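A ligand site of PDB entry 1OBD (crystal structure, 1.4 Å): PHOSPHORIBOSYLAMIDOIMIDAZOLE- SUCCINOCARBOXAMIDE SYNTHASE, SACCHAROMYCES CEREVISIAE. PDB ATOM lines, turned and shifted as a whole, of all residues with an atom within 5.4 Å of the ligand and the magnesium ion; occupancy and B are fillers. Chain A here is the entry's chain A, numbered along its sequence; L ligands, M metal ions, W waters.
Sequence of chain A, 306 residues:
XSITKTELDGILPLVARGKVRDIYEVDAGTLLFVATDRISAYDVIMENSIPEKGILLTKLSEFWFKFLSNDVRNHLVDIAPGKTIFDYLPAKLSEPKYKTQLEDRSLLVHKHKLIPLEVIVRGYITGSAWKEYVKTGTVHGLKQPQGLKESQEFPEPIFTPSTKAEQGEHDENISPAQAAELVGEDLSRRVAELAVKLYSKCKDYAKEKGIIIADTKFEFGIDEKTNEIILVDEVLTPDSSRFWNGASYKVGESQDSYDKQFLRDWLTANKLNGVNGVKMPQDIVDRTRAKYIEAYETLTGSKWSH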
ATOM      1  N   ALA A  16       6.206  19.742  26.327  1.00  0.00           N
ATOM      2  CA  ALA A  16       6.617  20.467  27.494  1.00  0.00           C
ATOM      3  C   ALA A  16       7.671  21.485  27.149  1.00  0.00           C
ATOM      4  O   ALA A  16       8.356  21.289  26.199  1.00  0.00           O
ATOM      5  CB  ALA A  16       7.230  19.497  28.499  1.00  0.00           C
ATOM      6  N   ARG A  17       7.806  22.575  27.917  1.00  0.00           N
ATOM      7  CA  ARG A  17       9.073  23.336  27.993  1.00  0.00           C
ATOM      8  C   ARG A  17       9.613  23.344  29.399  1.00  0.00           C
ATOM      9  O   ARG A  17       8.892  23.804  30.326  1.00  0.00           O
ATOM     10  CB  ARG A  17       8.985  24.767  27.457  1.00  0.00           C
ATOM     11  CG  ARG A  17       8.901  24.868  25.931  1.00  0.00           C
ATOM     12  CD  ARG A  17       9.302  26.243  25.347  1.00  0.00           C
ATOM     13  NE  ARG A  17       8.834  26.437  23.966  1.00  0.00           N
ATOM     14  CZ  ARG A  17       7.761  27.139  23.593  1.00  0.00           C
ATOM     15  NH1 ARG A  17       7.448  27.229  22.323  1.00  0.00           N
ATOM     16  NH2 ARG A  17       7.021  27.765  24.493  1.00  0.00           N
ATOM     17  N   GLY A  18      10.813  22.849  29.641  1.00  0.00           N
ATOM     18  CA  GLY A  18      11.487  22.863  30.922  1.00  0.00           C
ATOM     19  C   GLY A  18      12.274  24.163  31.078  1.00  0.00           C
ATOM     20  O   GLY A  18      12.076  25.098  30.294  1.00  0.00           O
ATOM     21  N   LYS A  19      13.200  24.186  32.013  1.00  0.00           N
ATOM     22  CA  LYS A  19      14.053  25.350  32.215  1.00  0.00           C
ATOM     23  C   LYS A  19      14.869  25.605  30.958  1.00  0.00           C
ATOM     24  O   LYS A  19      15.134  26.736  30.564  1.00  0.00           O
ATOM     25  CB  LYS A  19      15.027  25.140  33.401  1.00  0.00           C
ATOM     26  CG  LYS A  19      14.404  24.985  34.782  1.00  0.00           C
ATOM     27  CD  LYS A  19      13.726  26.264  35.252  1.00  0.00           C
ATOM     28  CE  LYS A  19      12.207  26.233  34.993  1.00  0.00           C
ATOM     29  NZ  LYS A  19      11.381  25.669  36.121  1.00  0.00           N
ATOM     30  N   VAL A  20      15.265  24.537  30.312  1.00  0.00           N
ATOM     31  CA  VAL A  20      16.249  24.620  29.261  1.00  0.00           C
ATOM     32  C   VAL A  20      15.833  23.891  27.999  1.00  0.00           C
ATOM     33  O   VAL A  20      16.238  24.254  26.916  1.00  0.00           O
ATOM     34  CB  VAL A  20      17.603  24.059  29.746  1.00  0.00           C
ATOM     35  CG1 VAL A  20      18.604  23.874  28.619  1.00  0.00           C
ATOM     36  CG2 VAL A  20      18.163  24.872  30.873  1.00  0.00           C
ATOM     37  N   ARG A  21      15.008  22.886  28.088  1.00  0.00           N
ATOM     38  CA  ARG A  21      14.654  22.070  26.926  1.00  0.00           C
ATOM     39  C   ARG A  21      13.195  22.244  26.508  1.00  0.00           C
ATOM     40  O   ARG A  21      12.315  22.430  27.337  1.00  0.00           O
ATOM     41  CB  ARG A  21      14.950  20.631  27.257  1.00  0.00           C
ATOM     42  CG  ARG A  21      16.476  20.406  27.497  1.00  0.00           C
ATOM     43  CD  ARG A  21      16.925  18.949  27.549  1.00  0.00           C
ATOM     44  NE  ARG A  21      16.205  18.164  28.537  1.00  0.00           N
ATOM     45  CZ  ARG A  21      16.435  16.853  28.735  1.00  0.00           C
ATOM     46  NH1 ARG A  21      17.330  16.194  28.023  1.00  0.00           N
ATOM     47  NH2 ARG A  21      15.735  16.229  29.631  1.00  0.00           N
ATOM     48  N   ILE A  23      10.344  20.157  24.394  1.00  0.00           N
ATOM     49  CA  ILE A  23      10.038  18.776  24.031  1.00  0.00           C
ATOM     50  C   ILE A  23       8.830  18.749  23.108  1.00  0.00           C
ATOM     51  O   ILE A  23       7.766  19.257  23.469  1.00  0.00           O
ATOM     52  CB  ILE A  23       9.707  17.938  25.265  1.00  0.00           C
ATOM     53  CG1 ILE A  23      10.783  18.045  26.325  1.00  0.00           C
ATOM     54  CG2 ILE A  23       9.459  16.508  24.858  1.00  0.00           C
ATOM     55  CD1 ILE A  23      10.649  17.026  27.389  1.00  0.00           C
ATOM     56  N   LEU A  31       9.650  11.277  20.603  1.00  0.00           N
ATOM     57  CA  LEU A  31       9.759  12.664  21.038  1.00  0.00           C
ATOM     58  C   LEU A  31      11.007  13.290  20.463  1.00  0.00           C
ATOM     59  O   LEU A  31      11.950  12.599  20.073  1.00  0.00           O
ATOM     60  CB  LEU A  31       9.819  12.762  22.555  1.00  0.00           C
ATOM     61  CG  LEU A  31       8.626  12.191  23.305  1.00  0.00           C
ATOM     62  CD1 LEU A  31       8.913  12.194  24.851  1.00  0.00           C
ATOM     63  CD2 LEU A  31       7.360  12.969  23.006  1.00  0.00           C
ATOM     64  N   PHE A  33      13.719  16.150  21.663  1.00  0.00           N
ATOM     65  CA  PHE A  33      14.251  16.922  22.794  1.00  0.00           C
ATOM     66  C   PHE A  33      15.163  17.998  22.261  1.00  0.00           C
ATOM     67  O   PHE A  33      16.229  17.662  21.745  1.00  0.00           O
ATOM     68  CB  PHE A  33      15.065  16.050  23.747  1.00  0.00           C
ATOM     69  CG  PHE A  33      14.271  15.193  24.705  1.00  0.00           C
ATOM     70  CD1 PHE A  33      14.869  14.733  25.847  1.00  0.00           C
ATOM     71  CD2 PHE A  33      12.988  14.785  24.481  1.00  0.00           C
ATOM     72  CE1 PHE A  33      14.192  13.934  26.750  1.00  0.00           C
ATOM     73  CE2 PHE A  33      12.303  14.006  25.386  1.00  0.00           C
ATOM     74  CZ  PHE A  33      12.892  13.600  26.534  1.00  0.00           C
ATOM     75  N   HIS A  75      17.370   5.767  25.468  1.00  0.00           N
ATOM     76  CA  HIS A  75      16.180   6.151  24.702  1.00  0.00           C
ATOM     77  C   HIS A  75      16.449   6.668  23.307  1.00  0.00           C
ATOM     78  O   HIS A  75      15.502   6.987  22.599  1.00  0.00           O
ATOM     79  CB  HIS A  75      15.305   7.171  25.476  1.00  0.00           C
ATOM     80  CG  HIS A  75      15.952   8.524  25.734  1.00  0.00           C
ATOM     81  ND1 HIS A  75      15.265   9.570  26.321  1.00  0.00           N
ATOM     82  CD2 HIS A  75      17.205   8.980  25.491  1.00  0.00           C
ATOM     83  CE1 HIS A  75      16.067  10.619  26.412  1.00  0.00           C
ATOM     84  NE2 HIS A  75      17.251  10.305  25.920  1.00  0.00           N
ATOM     85  N   VAL A 109      14.087  10.679  20.365  1.00  0.00           N
ATOM     86  CA  VAL A 109      14.067   9.684  21.429  1.00  0.00           C
ATOM     87  C   VAL A 109      12.780   8.876  21.430  1.00  0.00           C
ATOM     88  O   VAL A 109      11.714   9.371  21.076  1.00  0.00           O
ATOM     89  CB  VAL A 109      14.357  10.305  22.813  1.00  0.00           C
ATOM     90  CG1 VAL A 109      15.613  11.114  22.824  1.00  0.00           C
ATOM     91  CG2 VAL A 109      13.199  11.123  23.321  1.00  0.00           C
ATOM     92  N   HIS A 110      12.917   7.608  21.797  1.00  0.00           N
ATOM     93  CA  HIS A 110      11.756   6.759  21.993  1.00  0.00           C
ATOM     94  C   HIS A 110      11.041   7.153  23.274  1.00  0.00           C
ATOM     95  O   HIS A 110      11.687   7.341  24.331  1.00  0.00           O
ATOM     96  CB  HIS A 110      12.232   5.293  22.145  1.00  0.00           C
ATOM     97  CG  HIS A 110      12.827   4.697  20.907  1.00  0.00           C
ATOM     98  ND1 HIS A 110      12.094   4.421  19.784  1.00  0.00           N
ATOM     99  CD2 HIS A 110      14.105   4.303  20.632  1.00  0.00           C
ATOM    100  CE1 HIS A 110      12.888   3.912  18.855  1.00  0.00           C
ATOM    101  NE2 HIS A 110      14.106   3.825  19.337  1.00  0.00           N
ATOM    102  N   LYS A 111       9.713   7.239  23.190  1.00  0.00           N
ATOM    103  CA  LYS A 111       8.852   7.377  24.344  1.00  0.00           C
ATOM    104  C   LYS A 111       8.910   6.147  25.129  1.00  0.00           C
ATOM    105  O   LYS A 111       8.639   5.056  24.614  1.00  0.00           O
ATOM    106  CB  LYS A 111       7.416   7.440  23.921  1.00  0.00           C
ATOM    107  CG  LYS A 111       7.021   8.748  23.596  1.00  0.00           C
ATOM    108  CD  LYS A 111       5.490   8.805  23.445  1.00  0.00           C
ATOM    109  CE  LYS A 111       5.105  10.032  22.682  1.00  0.00           C
ATOM    110  NZ  LYS A 111       3.669   9.957  22.317  1.00  0.00           N
ATOM    111  N   HIS A 112       9.242   6.282  26.395  1.00  0.00           N
ATOM    112  CA  HIS A 112       9.237   5.143  27.250  1.00  0.00           C
ATOM    113  C   HIS A 112       8.307   5.393  28.419  1.00  0.00           C
ATOM    114  O   HIS A 112       7.982   6.539  28.764  1.00  0.00           O
ATOM    115  CB  HIS A 112      10.671   4.861  27.749  1.00  0.00           C
ATOM    116  CG  HIS A 112      11.480   4.069  26.752  1.00  0.00           C
ATOM    117  ND1 HIS A 112      11.262   2.741  26.494  1.00  0.00           N
ATOM    118  CD2 HIS A 112      12.497   4.439  25.953  1.00  0.00           C
ATOM    119  CE1 HIS A 112      12.102   2.319  25.583  1.00  0.00           C
ATOM    120  NE2 HIS A 112      12.883   3.328  25.239  1.00  0.00           N
ATOM    121  N   LEU A 114       8.198   5.940  32.027  1.00  0.00           N
ATOM    122  CA  LEU A 114       9.206   6.364  32.949  1.00  0.00           C
ATOM    123  C   LEU A 114       8.883   5.755  34.289  1.00  0.00           C
ATOM    124  O   LEU A 114       7.760   5.443  34.648  1.00  0.00           O
ATOM    125  CB  LEU A 114       9.365   7.905  33.068  1.00  0.00           C
ATOM    126  CG  LEU A 114      10.479   8.571  32.221  1.00  0.00           C
ATOM    127  CD1 LEU A 114      11.755   8.705  33.112  1.00  0.00           C
ATOM    128  CD2 LEU A 114      10.674   7.928  30.808  1.00  0.00           C
ATOM    129  N   LYS A 217      21.821  13.526  38.662  1.00  0.00           N
ATOM    130  CA  LYS A 217      20.433  13.118  38.638  1.00  0.00           C
ATOM    131  C   LYS A 217      20.149  12.394  37.351  1.00  0.00           C
ATOM    132  O   LYS A 217      20.208  12.978  36.262  1.00  0.00           O
ATOM    133  CB  LYS A 217      19.526  14.336  38.768  1.00  0.00           C
ATOM    134  CG  LYS A 217      18.081  13.990  38.865  1.00  0.00           C
ATOM    135  CD  LYS A 217      17.220  15.252  39.187  1.00  0.00           C
ATOM    136  CE  LYS A 217      17.336  16.339  38.144  1.00  0.00           C
ATOM    137  NZ  LYS A 217      16.695  15.907  36.867  1.00  0.00           N
ATOM    138  N   GLU A 219      17.263   9.938  35.226  1.00  0.00           N
ATOM    139  CA  GLU A 219      15.931   9.385  35.140  1.00  0.00           C
ATOM    140  C   GLU A 219      15.987   8.147  34.263  1.00  0.00           C
ATOM    141  O   GLU A 219      16.773   8.049  33.305  1.00  0.00           O
ATOM    142  CB  GLU A 219      14.924  10.393  34.595  1.00  0.00           C
ATOM    143  CG  GLU A 219      14.614  11.554  35.536  1.00  0.00           C
ATOM    144  CD  GLU A 219      13.568  12.495  34.978  1.00  0.00           C
ATOM    145  OE1 GLU A 219      13.358  13.572  35.584  1.00  0.00           O
ATOM    146  OE2 GLU A 219      12.985  12.183  33.907  1.00  0.00           O
ATOM    147  N   VAL A 232      17.180   7.480  30.272  1.00  0.00           N
ATOM    148  CA  VAL A 232      16.433   8.490  29.553  1.00  0.00           C
ATOM    149  C   VAL A 232      16.873   9.860  30.021  1.00  0.00           C
ATOM    150  O   VAL A 232      17.862  10.021  30.692  1.00  0.00           O
ATOM    151  CB  VAL A 232      14.910   8.285  29.672  1.00  0.00           C
ATOM    152  CG1 VAL A 232      14.473   6.849  29.239  1.00  0.00           C
ATOM    153  CG2 VAL A 232      14.400   8.562  31.114  1.00  0.00           C
ATOM    154  N   ASP A 233      16.110  10.865  29.647  1.00  0.00           N
ATOM    155  CA  ASP A 233      16.358  12.254  30.105  1.00  0.00           C
ATOM    156  C   ASP A 233      17.793  12.778  29.840  1.00  0.00           C
ATOM    157  O   ASP A 233      18.490  12.381  28.879  1.00  0.00           O
ATOM    158  CB  ASP A 233      15.980  12.300  31.588  1.00  0.00           C
ATOM    159  CG  ASP A 233      15.591  13.667  32.081  1.00  0.00           C
ATOM    160  OD1 ASP A 233      14.705  14.283  31.454  1.00  0.00           O
ATOM    161  OD2 ASP A 233      16.107  14.132  33.117  1.00  0.00           O
HETATM  162  P1  LIG L   1      13.697  20.706  34.147  1.00  0.00           P
HETATM  163  O1  LIG L   1      14.350  21.762  33.320  1.00  0.00           O
HETATM  164  O2  LIG L   1      14.370  19.328  33.966  1.00  0.00           O
HETATM  165  O3  LIG L   1      13.747  21.136  35.612  1.00  0.00           O
HETATM  166  P2  LIG L   1      11.476  19.428  32.960  1.00  0.00           P
HETATM  167  O4  LIG L   1      10.039  19.731  32.823  1.00  0.00           O
HETATM  168  O5  LIG L   1      11.790  18.079  33.598  1.00  0.00           O
HETATM  169  O6  LIG L   1      12.129  20.632  33.754  1.00  0.00           O
HETATM  170  P3  LIG L   1      12.997  18.477  30.715  1.00  0.00           P
HETATM  171  O7  LIG L   1      13.822  19.227  29.748  1.00  0.00           O
HETATM  172  O8  LIG L   1      13.823  17.647  31.679  1.00  0.00           O
HETATM  173  O9  LIG L   1      12.144  19.550  31.524  1.00  0.00           O
HETATM  174  O10 LIG L   1      11.899  17.631  29.941  1.00  0.00           O
HETATM  175  C1  LIG L   1      12.040  16.228  29.861  1.00  0.00           C
HETATM  176  C2  LIG L   1      10.696  15.595  30.150  1.00  0.00           C
HETATM  177  O11 LIG L   1      10.631  14.358  29.487  1.00  0.00           O
HETATM  178  C3  LIG L   1      10.571  15.287  31.610  1.00  0.00           C
HETATM  179  O12 LIG L   1       9.178  15.324  31.919  1.00  0.00           O
HETATM  180  C4  LIG L   1      11.198  13.891  31.711  1.00  0.00           C
HETATM  181  O13 LIG L   1      10.855  13.103  32.798  1.00  0.00           O
HETATM  182  C5  LIG L   1      10.638  13.292  30.438  1.00  0.00           C
HETATM  183  N1  LIG L   1      11.386  12.262  29.696  1.00  0.00           N
HETATM  184  C6  LIG L   1      12.750  12.172  29.692  1.00  0.00           C
HETATM  185  N2  LIG L   1      13.074  11.188  28.869  1.00  0.00           N
HETATM  186  C7  LIG L   1      11.965  10.588  28.349  1.00  0.00           C
HETATM  187  C8  LIG L   1      11.674   9.530  27.476  1.00  0.00           C
HETATM  188  N3  LIG L   1      12.542   8.896  26.716  1.00  0.00           N
HETATM  189  N4  LIG L   1      10.368   9.225  27.210  1.00  0.00           N
HETATM  190  C9  LIG L   1       9.342   9.944  27.754  1.00  0.00           C
HETATM  191  N5  LIG L   1       9.593  10.976  28.606  1.00  0.00           N
HETATM  192  C10 LIG L   1      10.882  11.291  28.891  1.00  0.00           C
HETATM  193 MG    MG M   1      13.864  17.424  33.683  1.00  0.00          MG
HETATM  194  O   HOH W   1      14.817  21.526  30.762  1.00  0.00           O
HETATM  195  O   HOH W   2       7.351  16.393  29.974  1.00  0.00           O
HETATM  196  O   HOH W   3       8.127  14.851  28.121  1.00  0.00           O
HETATM  197  O   HOH W   4       8.278  17.723  32.120  1.00  0.00           O
HETATM  198  O   HOH W   5       6.403   8.898  28.525  1.00  0.00           O
HETATM  199  O   HOH W   6       7.201  11.247  29.855  1.00  0.00           O
HETATM  200  O   HOH W   7      13.410  15.563  33.517  1.00  0.00           O
HETATM  201  O   HOH W   8      10.127  16.140  35.008  1.00  0.00           O
HETATM  202  O   HOH W   9       7.784  21.618  32.126  1.00  0.00           O
HETATM  203  O   HOH W  10      17.209  22.249  33.890  1.00  0.00           O
HETATM  204  O   HOH W  11      12.373  19.132  36.970  1.00  0.00           O
HETATM  205  O   HOH W  12      11.404  22.617  36.114  1.00  0.00           O
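An oxygen (O13) of the ligand is in hydrogen-bond range of the side-chain carboxylate (OE2) of Glu 219, 2.6 Å away.
The backbone NH (N) of Asp 233 lies within hydrogen-bond range of a nitrogen (N2) of the ligand.
The backbone carbonyl oxygen (O) of His 110 lies within hydrogen-bond range of a nitrogen (N3) of the ligand (3.0 Å).
O1 of the ligand sits at hydrogen-bond distance from N of Lys 19, at 3.0 Å.
A nitrogen (N4) of the ligand sits at hydrogen-bond distance from the backbone NH (N) of His 112 (3.3 Å).
A nitrogen (N3) of the ligand is in hydrogen-bond range of a ring nitrogen (ND1) of His 75.
O7 of the ligand is in salt-bridge range of NE of Arg 21, 2.9 Å away.
The side-chain carboxylate (OD1) of Asp 233 is in salt-bridge range of the guanidinium group (NH2) of Arg 21, at 2.9 Å.
O of Ala 16 sits at hydrogen-bond distance from N of Ile 23 (2.9 Å).
O of Glu 219 is in hydrogen-bond range of N of Val 232, at 3.1 Å.
N of His 110 sits at hydrogen-bond distance from O of His 75 (2.8 Å).
The backbone carbonyl oxygen (O) of Val 109 lies within hydrogen-bond range of the backbone NH (N) of Leu 31 (2.8 Å).
Merely in contact with the ligand: Gly 18 (3.4 Å), Ile 23 (2.9 Å), Leu 31 (3.7 Å), Phe 33 (3.4 Å), Lys 111 (3.7 Å), Leu 114 (3.8 Å) and Val 232 (3.5 Å).
Hydrophobic or aromatic side chains that line the ligand: Ile 23, Leu 31, Phe 33, His 75, Leu 114 and Val 232.
Of the 19 residues printed, 14 come within 4 Å of the ligand.
The nearest printed residue that does not touch the ligand is Val 109 (4.1 Å).
Asp 233 touches the magnesium ion (OD1 to MG, 3.9 Å).
Of the 19 residues printed, 1 comes within 4 Å of the magnesium ion.
The nearest printed residue that does not touch the magnesium ion is Glu 219 (4.3 Å).
The magnesium ion is bound by water W7 (1.9 Å), an oxygen (O2) of the ligand (2.0 Å), an oxygen (O8) of the ligand (2.0 Å) and an oxygen (O5) of the ligand (2.2 Å).
Water W7 bridges OD1 of Asp 233 and OE1 of Glu 219.
Water W12 lies within hydrogen-bond range of O3 of the ligand (2.8 Å) and NZ of Lys 19 (3.1 Å).
Water W9 lies within hydrogen-bond range of an oxygen (O4) of the ligand and the backbone carbonyl oxygen of Arg 17.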
